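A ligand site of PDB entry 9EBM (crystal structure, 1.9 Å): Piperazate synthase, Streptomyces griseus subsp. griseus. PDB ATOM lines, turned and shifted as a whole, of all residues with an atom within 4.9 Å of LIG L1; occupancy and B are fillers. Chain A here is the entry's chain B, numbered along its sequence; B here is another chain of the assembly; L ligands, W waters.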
ATOM      1  N   LEU A  24      29.314  15.937 -12.761  1.00  0.00           N
ATOM      2  CA  LEU A  24      27.882  15.821 -12.490  1.00  0.00           C
ATOM      3  C   LEU A  24      27.687  16.217 -11.036  1.00  0.00           C
ATOM      4  O   LEU A  24      27.868  15.408 -10.122  1.00  0.00           O
ATOM      5  CB  LEU A  24      27.364  14.412 -12.768  1.00  0.00           C
ATOM      6  CG  LEU A  24      25.835  14.266 -12.716  1.00  0.00           C
ATOM      7  CD1 LEU A  24      25.155  14.845 -13.982  1.00  0.00           C
ATOM      8  CD2 LEU A  24      25.433  12.801 -12.506  1.00  0.00           C
ATOM      9  N   THR A  40      19.122  18.694  -7.526  1.00  0.00           N
ATOM     10  CA  THR A  40      19.126  18.076  -8.844  1.00  0.00           C
ATOM     11  C   THR A  40      20.555  17.747  -9.252  1.00  0.00           C
ATOM     12  O   THR A  40      21.443  18.595  -9.119  1.00  0.00           O
ATOM     13  CB  THR A  40      18.493  18.998  -9.899  1.00  0.00           C
ATOM     14  OG1 THR A  40      17.127  19.225  -9.570  1.00  0.00           O
ATOM     15  CG2 THR A  40      18.616  18.404 -11.325  1.00  0.00           C
ATOM     16  N   HIS A  41      20.766  16.539  -9.775  1.00  0.00           N
ATOM     17  CA  HIS A  41      22.041  16.150 -10.360  1.00  0.00           C
ATOM     18  C   HIS A  41      22.122  16.631 -11.788  1.00  0.00           C
ATOM     19  O   HIS A  41      21.254  16.293 -12.605  1.00  0.00           O
ATOM     20  CB  HIS A  41      22.192  14.638 -10.288  1.00  0.00           C
ATOM     21  CG  HIS A  41      22.094  14.120  -8.896  1.00  0.00           C
ATOM     22  ND1 HIS A  41      23.202  13.965  -8.084  1.00  0.00           N
ATOM     23  CD2 HIS A  41      21.021  13.750  -8.146  1.00  0.00           C
ATOM     24  CE1 HIS A  41      22.816  13.495  -6.913  1.00  0.00           C
ATOM     25  NE2 HIS A  41      21.502  13.381  -6.912  1.00  0.00           N
ATOM     26  N   LEU A  42      23.151  17.410 -12.121  1.00  0.00           N
ATOM     27  CA  LEU A  42      23.209  18.034 -13.437  1.00  0.00           C
ATOM     28  C   LEU A  42      24.664  18.322 -13.781  1.00  0.00           C
ATOM     29  O   LEU A  42      25.505  18.475 -12.880  1.00  0.00           O
ATOM     30  CB  LEU A  42      22.370  19.327 -13.472  1.00  0.00           C
ATOM     31  CG  LEU A  42      22.560  20.367 -12.371  1.00  0.00           C
ATOM     32  CD1 LEU A  42      23.747  21.256 -12.683  1.00  0.00           C
ATOM     33  CD2 LEU A  42      21.301  21.224 -12.215  1.00  0.00           C
ATOM     34  N   PRO A  43      24.984  18.436 -15.074  1.00  0.00           N
ATOM     35  CA  PRO A  43      26.373  18.666 -15.483  1.00  0.00           C
ATOM     36  C   PRO A  43      26.772  20.144 -15.406  1.00  0.00           C
ATOM     37  O   PRO A  43      26.037  21.035 -15.831  1.00  0.00           O
ATOM     38  CB  PRO A  43      26.374  18.194 -16.939  1.00  0.00           C
ATOM     39  CG  PRO A  43      24.989  18.517 -17.428  1.00  0.00           C
ATOM     40  CD  PRO A  43      24.085  18.246 -16.241  1.00  0.00           C
ATOM     41  N   HIS A  66      22.788  23.007 -16.759  1.00  0.00           N
ATOM     42  CA  HIS A  66      21.437  23.002 -17.277  1.00  0.00           C
ATOM     43  C   HIS A  66      20.648  21.918 -16.567  1.00  0.00           C
ATOM     44  O   HIS A  66      21.211  20.953 -16.036  1.00  0.00           O
ATOM     45  CB  HIS A  66      21.401  22.844 -18.820  1.00  0.00           C
ATOM     46  CG  HIS A  66      21.646  21.462 -19.342  1.00  0.00           C
ATOM     47  ND1 HIS A  66      22.911  20.932 -19.500  1.00  0.00           N
ATOM     48  CD2 HIS A  66      20.783  20.518 -19.797  1.00  0.00           C
ATOM     49  CE1 HIS A  66      22.817  19.724 -20.022  1.00  0.00           C
ATOM     50  NE2 HIS A  66      21.540  19.445 -20.212  1.00  0.00           N
ATOM     51  N   MET A  67      19.334  22.119 -16.527  1.00  0.00           N
ATOM     52  CA  MET A  67      18.411  21.165 -15.959  1.00  0.00           C
ATOM     53  C   MET A  67      17.191  21.103 -16.874  1.00  0.00           C
ATOM     54  O   MET A  67      17.110  21.807 -17.884  1.00  0.00           O
ATOM     55  CB  MET A  67      18.034  21.545 -14.525  1.00  0.00           C
ATOM     56  CG  MET A  67      17.201  22.800 -14.421  1.00  0.00           C
ATOM     57  SD  MET A  67      16.774  23.183 -12.696  1.00  0.00           S
ATOM     58  CE  MET A  67      18.394  23.424 -12.005  1.00  0.00           C
ATOM     59  N   ASN A  68      16.245  20.242 -16.498  1.00  0.00           N
ATOM     60  CA  ASN A  68      14.970  20.177 -17.193  1.00  0.00           C
ATOM     61  C   ASN A  68      14.092  21.344 -16.756  1.00  0.00           C
ATOM     62  O   ASN A  68      13.961  21.622 -15.557  1.00  0.00           O
ATOM     63  CB  ASN A  68      14.291  18.847 -16.886  1.00  0.00           C
ATOM     64  CG  ASN A  68      13.072  18.586 -17.762  1.00  0.00           C
ATOM     65  OD1 ASN A  68      12.400  19.508 -18.204  1.00  0.00           O
ATOM     66  ND2 ASN A  68      12.784  17.303 -17.995  1.00  0.00           N
ATOM     67  N   ASN A  71      11.512  20.494 -14.303  1.00  0.00           N
ATOM     68  CA  ASN A  71      11.975  20.314 -12.935  1.00  0.00           C
ATOM     69  C   ASN A  71      11.480  21.458 -12.076  1.00  0.00           C
ATOM     70  O   ASN A  71      11.790  22.630 -12.378  1.00  0.00           O
ATOM     71  CB  ASN A  71      13.500  20.253 -12.921  1.00  0.00           C
ATOM     72  CG  ASN A  71      14.078  19.864 -11.580  1.00  0.00           C
ATOM     73  OD1 ASN A  71      13.534  20.188 -10.519  1.00  0.00           O
ATOM     74  ND2 ASN A  71      15.220  19.185 -11.615  1.00  0.00           N
ATOM     75  N   VAL A 132      24.475  23.842 -23.817  1.00  0.00           N
ATOM     76  CA  VAL A 132      24.418  22.386 -23.897  1.00  0.00           C
ATOM     77  C   VAL A 132      25.387  21.881 -24.947  1.00  0.00           C
ATOM     78  O   VAL A 132      25.995  20.806 -24.776  1.00  0.00           O
ATOM     79  CB  VAL A 132      22.976  21.900 -24.145  1.00  0.00           C
ATOM     80  CG1 VAL A 132      22.118  22.186 -22.931  1.00  0.00           C
ATOM     81  CG2 VAL A 132      22.383  22.571 -25.399  1.00  0.00           C
ATOM     82  N   ARG A 133      25.585  22.626 -26.026  1.00  0.00           N
ATOM     83  CA  ARG A 133      26.573  22.218 -27.022  1.00  0.00           C
ATOM     84  C   ARG A 133      27.981  22.275 -26.449  1.00  0.00           C
ATOM     85  O   ARG A 133      28.813  21.413 -26.776  1.00  0.00           O
ATOM     86  CB  ARG A 133      26.459  23.089 -28.273  1.00  0.00           C
ATOM     87  CG  ARG A 133      25.343  22.653 -29.175  1.00  0.00           C
ATOM     88  CD  ARG A 133      25.098  23.686 -30.274  1.00  0.00           C
ATOM     89  NE  ARG A 133      26.091  23.583 -31.338  1.00  0.00           N
ATOM     90  CZ  ARG A 133      26.144  24.400 -32.375  1.00  0.00           C
ATOM     91  NH1 ARG A 133      27.078  24.236 -33.302  1.00  0.00           N
ATOM     92  NH2 ARG A 133      25.269  25.393 -32.495  1.00  0.00           N
ATOM     93  N   THR A 135      28.656  21.824 -23.224  1.00  0.00           N
ATOM     94  CA  THR A 135      28.715  20.694 -22.326  1.00  0.00           C
ATOM     95  C   THR A 135      28.976  19.399 -23.089  1.00  0.00           C
ATOM     96  O   THR A 135      29.861  18.615 -22.720  1.00  0.00           O
ATOM     97  CB  THR A 135      27.418  20.591 -21.529  1.00  0.00           C
ATOM     98  OG1 THR A 135      27.196  21.829 -20.827  1.00  0.00           O
ATOM     99  CG2 THR A 135      27.515  19.467 -20.518  1.00  0.00           C
ATOM    100  N   ALA A 136      28.227  19.184 -24.178  1.00  0.00           N
ATOM    101  CA  ALA A 136      28.405  17.988 -25.002  1.00  0.00           C
ATOM    102  C   ALA A 136      29.822  17.878 -25.527  1.00  0.00           C
ATOM    103  O   ALA A 136      30.471  16.833 -25.385  1.00  0.00           O
ATOM    104  CB  ALA A 136      27.401  17.990 -26.160  1.00  0.00           C
ATOM    105  N   PHE A 139      32.499  17.306 -22.553  1.00  0.00           N
ATOM    106  CA  PHE A 139      32.481  15.983 -21.925  1.00  0.00           C
ATOM    107  C   PHE A 139      32.910  14.904 -22.918  1.00  0.00           C
ATOM    108  O   PHE A 139      33.625  13.960 -22.550  1.00  0.00           O
ATOM    109  CB  PHE A 139      31.092  15.670 -21.368  1.00  0.00           C
ATOM    110  CG  PHE A 139      30.746  16.392 -20.099  1.00  0.00           C
ATOM    111  CD1 PHE A 139      31.512  17.456 -19.626  1.00  0.00           C
ATOM    112  CD2 PHE A 139      29.635  16.016 -19.365  1.00  0.00           C
ATOM    113  CE1 PHE A 139      31.175  18.115 -18.440  1.00  0.00           C
ATOM    114  CE2 PHE A 139      29.285  16.657 -18.179  1.00  0.00           C
ATOM    115  CZ  PHE A 139      30.054  17.725 -17.719  1.00  0.00           C
ATOM    116  N   PHE A 156      19.365  18.803 -31.527  1.00  0.00           N
ATOM    117  CA  PHE A 156      19.572  19.692 -30.385  1.00  0.00           C
ATOM    118  C   PHE A 156      18.602  20.875 -30.436  1.00  0.00           C
ATOM    119  O   PHE A 156      18.016  21.246 -29.413  1.00  0.00           O
ATOM    120  CB  PHE A 156      21.005  20.223 -30.328  1.00  0.00           C
ATOM    121  CG  PHE A 156      22.054  19.187 -30.034  1.00  0.00           C
ATOM    122  CD1 PHE A 156      21.745  17.859 -29.888  1.00  0.00           C
ATOM    123  CD2 PHE A 156      23.394  19.575 -29.929  1.00  0.00           C
ATOM    124  CE1 PHE A 156      22.727  16.927 -29.651  1.00  0.00           C
ATOM    125  CE2 PHE A 156      24.379  18.652 -29.688  1.00  0.00           C
ATOM    126  CZ  PHE A 156      24.046  17.319 -29.540  1.00  0.00           C
ATOM    127  N   ILE A 159      14.933  19.846 -29.246  1.00  0.00           N
ATOM    128  CA  ILE A 159      14.658  19.572 -27.843  1.00  0.00           C
ATOM    129  C   ILE A 159      15.108  20.689 -26.900  1.00  0.00           C
ATOM    130  O   ILE A 159      14.694  20.698 -25.729  1.00  0.00           O
ATOM    131  CB  ILE A 159      15.278  18.224 -27.391  1.00  0.00           C
ATOM    132  CG1 ILE A 159      16.803  18.328 -27.284  1.00  0.00           C
ATOM    133  CG2 ILE A 159      14.915  17.116 -28.369  1.00  0.00           C
ATOM    134  CD1 ILE A 159      17.463  17.077 -26.671  1.00  0.00           C
ATOM    135  N   VAL A 160      15.894  21.654 -27.384  1.00  0.00           N
ATOM    136  CA  VAL A 160      16.481  22.671 -26.522  1.00  0.00           C
ATOM    137  C   VAL A 160      15.466  23.546 -25.783  1.00  0.00           C
ATOM    138  O   VAL A 160      15.803  24.032 -24.691  1.00  0.00           O
ATOM    139  CB  VAL A 160      17.480  23.554 -27.300  1.00  0.00           C
ATOM    140  CG1 VAL A 160      16.771  24.652 -28.100  1.00  0.00           C
ATOM    141  CG2 VAL A 160      18.493  24.174 -26.340  1.00  0.00           C
ATOM    142  N   GLY A 162      13.222  22.699 -23.920  1.00  0.00           N
ATOM    143  CA  GLY A 162      13.064  22.087 -22.618  1.00  0.00           C
ATOM    144  C   GLY A 162      14.245  22.265 -21.690  1.00  0.00           C
ATOM    145  O   GLY A 162      14.152  21.875 -20.521  1.00  0.00           O
ATOM    146  N   VAL A 163      15.336  22.849 -22.181  1.00  0.00           N
ATOM    147  CA  VAL A 163      16.527  23.031 -21.370  1.00  0.00           C
ATOM    148  C   VAL A 163      16.400  24.295 -20.534  1.00  0.00           C
ATOM    149  O   VAL A 163      16.142  25.381 -21.068  1.00  0.00           O
ATOM    150  CB  VAL A 163      17.790  23.098 -22.258  1.00  0.00           C
ATOM    151  CG1 VAL A 163      19.012  23.345 -21.378  1.00  0.00           C
ATOM    152  CG2 VAL A 163      17.951  21.831 -23.052  1.00  0.00           C
ATOM    153  N   PHE B   2      12.834  15.362  -8.751  1.00  0.00           N
ATOM    154  CA  PHE B   2      12.286  15.343 -10.109  1.00  0.00           C
ATOM    155  C   PHE B   2      12.832  14.134 -10.851  1.00  0.00           C
ATOM    156  O   PHE B   2      14.022  14.084 -11.166  1.00  0.00           O
ATOM    157  CB  PHE B   2      12.627  16.625 -10.859  1.00  0.00           C
ATOM    158  CG  PHE B   2      12.106  16.636 -12.262  1.00  0.00           C
ATOM    159  CD1 PHE B   2      10.752  16.811 -12.498  1.00  0.00           C
ATOM    160  CD2 PHE B   2      12.948  16.406 -13.336  1.00  0.00           C
ATOM    161  CE1 PHE B   2      10.242  16.814 -13.790  1.00  0.00           C
ATOM    162  CE2 PHE B   2      12.447  16.386 -14.633  1.00  0.00           C
ATOM    163  CZ  PHE B   2      11.087  16.592 -14.861  1.00  0.00           C
ATOM    164  N   TYR B  93      29.682   8.474 -17.803  1.00  0.00           N
ATOM    165  CA  TYR B  93      29.373   9.237 -18.991  1.00  0.00           C
ATOM    166  C   TYR B  93      29.041   8.300 -20.145  1.00  0.00           C
ATOM    167  O   TYR B  93      29.714   7.293 -20.361  1.00  0.00           O
ATOM    168  CB  TYR B  93      30.561  10.110 -19.382  1.00  0.00           C
ATOM    169  CG  TYR B  93      30.364  10.814 -20.718  1.00  0.00           C
ATOM    170  CD1 TYR B  93      29.512  11.906 -20.827  1.00  0.00           C
ATOM    171  CD2 TYR B  93      31.010  10.367 -21.857  1.00  0.00           C
ATOM    172  CE1 TYR B  93      29.329  12.562 -22.063  1.00  0.00           C
ATOM    173  CE2 TYR B  93      30.830  11.009 -23.088  1.00  0.00           C
ATOM    174  CZ  TYR B  93      29.992  12.103 -23.181  1.00  0.00           C
ATOM    175  OH  TYR B  93      29.834  12.724 -24.399  1.00  0.00           O
ATOM    176  N   ALA B 105      22.275  12.506 -28.485  1.00  0.00           N
ATOM    177  CA  ALA B 105      22.819  13.506 -27.598  1.00  0.00           C
ATOM    178  C   ALA B 105      23.544  12.749 -26.495  1.00  0.00           C
ATOM    179  O   ALA B 105      23.055  11.701 -26.053  1.00  0.00           O
ATOM    180  CB  ALA B 105      21.719  14.391 -26.982  1.00  0.00           C
ATOM    181  N   PRO B 106      24.700  13.227 -26.045  1.00  0.00           N
ATOM    182  CA  PRO B 106      25.369  12.550 -24.935  1.00  0.00           C
ATOM    183  C   PRO B 106      24.558  12.714 -23.659  1.00  0.00           C
ATOM    184  O   PRO B 106      23.696  13.593 -23.549  1.00  0.00           O
ATOM    185  CB  PRO B 106      26.723  13.270 -24.821  1.00  0.00           C
ATOM    186  CG  PRO B 106      26.788  14.211 -25.977  1.00  0.00           C
ATOM    187  CD  PRO B 106      25.381  14.478 -26.411  1.00  0.00           C
ATOM    188  N   THR B 107      24.861  11.860 -22.685  1.00  0.00           N
ATOM    189  CA  THR B 107      24.241  11.980 -21.375  1.00  0.00           C
ATOM    190  C   THR B 107      25.159  11.344 -20.339  1.00  0.00           C
ATOM    191  O   THR B 107      26.214  10.789 -20.666  1.00  0.00           O
ATOM    192  CB  THR B 107      22.841  11.354 -21.373  1.00  0.00           C
ATOM    193  OG1 THR B 107      22.104  11.840 -20.237  1.00  0.00           O
ATOM    194  CG2 THR B 107      22.903   9.835 -21.332  1.00  0.00           C
ATOM    195  N   TRP B 108      24.741  11.428 -19.095  1.00  0.00           N
ATOM    196  CA  TRP B 108      25.465  10.810 -17.982  1.00  0.00           C
ATOM    197  C   TRP B 108      24.511   9.857 -17.292  1.00  0.00           C
ATOM    198  O   TRP B 108      23.477  10.287 -16.774  1.00  0.00           O
ATOM    199  CB  TRP B 108      25.989  11.863 -17.009  1.00  0.00           C
ATOM    200  CG  TRP B 108      27.206  11.407 -16.243  1.00  0.00           C
ATOM    201  CD1 TRP B 108      27.270  10.423 -15.295  1.00  0.00           C
ATOM    202  CD2 TRP B 108      28.545  11.894 -16.400  1.00  0.00           C
ATOM    203  NE1 TRP B 108      28.558  10.280 -14.837  1.00  0.00           N
ATOM    204  CE2 TRP B 108      29.364  11.170 -15.504  1.00  0.00           C
ATOM    205  CE3 TRP B 108      29.130  12.873 -17.205  1.00  0.00           C
ATOM    206  CZ2 TRP B 108      30.730  11.406 -15.393  1.00  0.00           C
ATOM    207  CZ3 TRP B 108      30.496  13.109 -17.094  1.00  0.00           C
ATOM    208  CH2 TRP B 108      31.275  12.380 -16.183  1.00  0.00           C
ATOM    209  N   PHE B 110      23.513   7.646 -14.199  1.00  0.00           N
ATOM    210  CA  PHE B 110      23.853   7.771 -12.786  1.00  0.00           C
ATOM    211  C   PHE B 110      22.685   7.260 -11.959  1.00  0.00           C
ATOM    212  O   PHE B 110      21.575   7.058 -12.457  1.00  0.00           O
ATOM    213  CB  PHE B 110      24.210   9.214 -12.406  1.00  0.00           C
ATOM    214  CG  PHE B 110      23.023  10.140 -12.322  1.00  0.00           C
ATOM    215  CD1 PHE B 110      22.531  10.755 -13.464  1.00  0.00           C
ATOM    216  CD2 PHE B 110      22.415  10.395 -11.098  1.00  0.00           C
ATOM    217  CE1 PHE B 110      21.438  11.624 -13.388  1.00  0.00           C
ATOM    218  CE2 PHE B 110      21.339  11.246 -11.016  1.00  0.00           C
ATOM    219  CZ  PHE B 110      20.841  11.865 -12.166  1.00  0.00           C
ATOM    220  N   MET B 176      16.468   7.859  -8.554  1.00  0.00           N
ATOM    221  CA  MET B 176      16.761   8.219  -9.937  1.00  0.00           C
ATOM    222  C   MET B 176      17.755   7.189 -10.456  1.00  0.00           C
ATOM    223  O   MET B 176      18.900   7.133 -10.005  1.00  0.00           O
ATOM    224  CB  MET B 176      17.332   9.638 -10.027  1.00  0.00           C
ATOM    225  CG  MET B 176      17.994   9.936 -11.344  1.00  0.00           C
ATOM    226  SD  MET B 176      16.797  10.514 -12.555  1.00  0.00           S
ATOM    227  CE  MET B 176      16.534  12.180 -11.983  1.00  0.00           C
ATOM    228  N   LYS B 178      19.070   6.585 -13.810  1.00  0.00           N
ATOM    229  CA  LYS B 178      19.181   7.050 -15.186  1.00  0.00           C
ATOM    230  C   LYS B 178      20.110   6.095 -15.903  1.00  0.00           C
ATOM    231  O   LYS B 178      21.334   6.218 -15.856  1.00  0.00           O
ATOM    232  CB  LYS B 178      19.689   8.488 -15.244  1.00  0.00           C
ATOM    233  CG  LYS B 178      19.780   9.055 -16.645  1.00  0.00           C
ATOM    234  CD  LYS B 178      20.069  10.552 -16.596  1.00  0.00           C
ATOM    235  CE  LYS B 178      19.730  11.260 -17.917  1.00  0.00           C
ATOM    236  NZ  LYS B 178      20.186  10.420 -19.060  1.00  0.00           N
HETATM  237  C1  LIG L   1      18.067  17.417 -18.986  1.00  0.00           C
HETATM  238  C2  LIG L   1      22.596  15.826 -18.659  1.00  0.00           C
HETATM  239  C3  LIG L   1      23.796  17.585 -23.049  1.00  0.00           C
HETATM  240  C4  LIG L   1      19.134  18.748 -23.582  1.00  0.00           C
HETATM  241  C5  LIG L   1      19.207  16.840 -18.478  1.00  0.00           C
HETATM  242  C6  LIG L   1      19.383  16.256 -17.156  1.00  0.00           C
HETATM  243  C7  LIG L   1      20.644  15.796 -17.063  1.00  0.00           C
HETATM  244  C8  LIG L   1      21.305  16.105 -18.317  1.00  0.00           C
HETATM  245  C9  LIG L   1      21.276  15.102 -15.839  1.00  0.00           C
HETATM  246  C10 LIG L   1      18.284  16.165 -16.077  1.00  0.00           C
HETATM  247  C11 LIG L   1      18.134  17.533 -15.400  1.00  0.00           C
HETATM  248  C12 LIG L   1      17.071  17.482 -14.340  1.00  0.00           C
HETATM  249  O1  LIG L   1      16.961  16.453 -13.628  1.00  0.00           O
HETATM  250  O2  LIG L   1      16.320  18.484 -14.206  1.00  0.00           O
HETATM  251  C13 LIG L   1      23.257  16.158 -19.817  1.00  0.00           C
HETATM  252  C14 LIG L   1      24.608  15.764 -20.062  1.00  0.00           C
HETATM  253  C15 LIG L   1      24.981  16.238 -21.235  1.00  0.00           C
HETATM  254  C16 LIG L   1      23.860  16.949 -21.835  1.00  0.00           C
HETATM  255  C17 LIG L   1      25.573  14.961 -19.157  1.00  0.00           C
HETATM  256  C18 LIG L   1      26.425  15.898 -21.688  1.00  0.00           C
HETATM  257  C19 LIG L   1      27.072  16.637 -22.551  1.00  0.00           C
HETATM  258  C20 LIG L   1      22.630  18.038 -23.620  1.00  0.00           C
HETATM  259  C21 LIG L   1      22.451  18.513 -24.974  1.00  0.00           C
HETATM  260  C22 LIG L   1      21.172  18.849 -25.135  1.00  0.00           C
HETATM  261  C23 LIG L   1      20.468  18.571 -23.872  1.00  0.00           C
HETATM  262  C24 LIG L   1      23.592  18.607 -26.000  1.00  0.00           C
HETATM  263  C25 LIG L   1      20.577  19.400 -26.455  1.00  0.00           C
HETATM  264  C26 LIG L   1      19.477  20.153 -26.481  1.00  0.00           C
HETATM  265  C27 LIG L   1      18.471  18.435 -22.412  1.00  0.00           C
HETATM  266  C28 LIG L   1      17.025  18.483 -22.260  1.00  0.00           C
HETATM  267  C29 LIG L   1      16.734  18.121 -21.004  1.00  0.00           C
HETATM  268  C30 LIG L   1      17.966  17.837 -20.306  1.00  0.00           C
HETATM  269  C31 LIG L   1      16.026  18.885 -23.377  1.00  0.00           C
HETATM  270  C32 LIG L   1      15.317  18.022 -20.375  1.00  0.00           C
HETATM  271  C33 LIG L   1      14.528  16.842 -20.938  1.00  0.00           C
HETATM  272  C34 LIG L   1      15.363  15.591 -21.056  1.00  0.00           C
HETATM  273  O3  LIG L   1      15.991  15.187 -20.039  1.00  0.00           O
HETATM  274  O4  LIG L   1      15.373  14.975 -22.157  1.00  0.00           O
HETATM  275  N1  LIG L   1      20.410  16.725 -19.130  1.00  0.00           N
HETATM  276  N2  LIG L   1      22.801  16.895 -20.932  1.00  0.00           N
HETATM  277  N3  LIG L   1      21.403  18.093 -22.997  1.00  0.00           N
HETATM  278  N4  LIG L   1      19.021  18.026 -21.185  1.00  0.00           N
HETATM  279 FE1  LIG L   1      20.949  17.552 -21.037  1.00  0.00          FE
HETATM  280  C1  LG2 L   2      18.401  12.264 -25.267  1.00  0.00           C
HETATM  281  N1  LG2 L   2      16.522  12.804 -23.643  1.00  0.00           N
HETATM  282  O1  LG2 L   2      18.524  11.308 -24.487  1.00  0.00           O
HETATM  283  C2  LG2 L   2      17.472  13.512 -24.607  1.00  0.00           C
HETATM  284  C3  LG2 L   2      18.327  14.583 -23.908  1.00  0.00           C
HETATM  285  C4  LG2 L   2      20.697  15.026 -23.063  1.00  0.00           C
HETATM  286  N2  LG2 L   2      20.414  15.719 -21.761  1.00  0.00           N
HETATM  287  C5  LG2 L   2      19.573  13.979 -23.248  1.00  0.00           C
HETATM  288  O2  LG2 L   2      20.401  14.724 -20.814  1.00  0.00           O
HETATM  289  O3  LG2 L   2      18.793  12.502 -26.407  1.00  0.00           O
HETATM  290  O   HOH W   1      19.052  14.734 -13.044  1.00  0.00           O
HETATM  291  O   HOH W   2      14.703  15.256 -17.490  1.00  0.00           O
HETATM  292  O   HOH W   3      18.347  13.436 -19.845  1.00  0.00           O
HETATM  293  O   HOH W   4      15.664  14.485 -14.958  1.00  0.00           O
HETATM  294  O   HOH W   5      16.081  15.702 -11.040  1.00  0.00           O
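N of Asn 68 lies within hydrogen-bond range of O2 of LIG L1 (2.9 Å).
O2 of LIG L1 sits at hydrogen-bond distance from ND2 of Asn 71 (2.9 Å).
OG1 of Thr 107 of chain B lies within hydrogen-bond range of O2 of LG2 L2 (3.4 Å).
A ring nitrogen (NE2) of His 66 binds an iron atom (FE1) of LIG L1, at 2.1 Å.
An iron atom (FE1) of LIG L1 is bound by a nitrogen (N2) of LG2 L2 (2.0 Å).
OG1 of Thr 40 is in hydrogen-bond range of ND2 of Asn 71, at 2.8 Å.
OG1 of Thr 107 of chain B sits at hydrogen-bond distance from NZ of Lys 178 of chain B.
Residues that only touch LIG L1: Ala 136 (3.1 Å), Ile 159 (3.3 Å), Val 163 (3.3 Å), Thr 135 (3.4 Å), Thr 40 (3.4 Å), His 41 (3.4 Å), Phe 156 (3.5 Å), Val 132 (3.5 Å), Met 67 (3.5 Å), Trp 108 of chain B (3.6 Å), Pro 43 (3.7 Å), Pro 106 of chain B (3.7 Å), Thr 107 of chain B (3.8 Å), Val 160 (3.9 Å) and Phe 139 (3.96 Å).
18 residues have an atom within 4 Å of LIG L1: Thr 40, His 41, Pro 43, His 66, Met 67, Asn 68, Asn 71, Val 132, Thr 135, Ala 136, Phe 139, Phe 156, Ile 159, Val 160, Val 163, Pro 106 of chain B, Thr 107 of chain B and Trp 108 of chain B.
Water W1 bridges the backbone carbonyl oxygen (O) of His 41 and an oxygen (O1) of LIG L1.
Water W5 lies within hydrogen-bond range of the backbone carbonyl oxygen (O) of Phe 2 of chain B and an oxygen (O1) of LIG L1.
Water W2 lies within hydrogen-bond range of the side-chain amide nitrogen of Asn 68 (2.9 Å) and an oxygen (O3) of LIG L1 (2.9 Å).
Water W3 lies within hydrogen-bond range of O2 of LG2 L2 (2.6 Å) and O3 of LIG L1 (2.9 Å).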
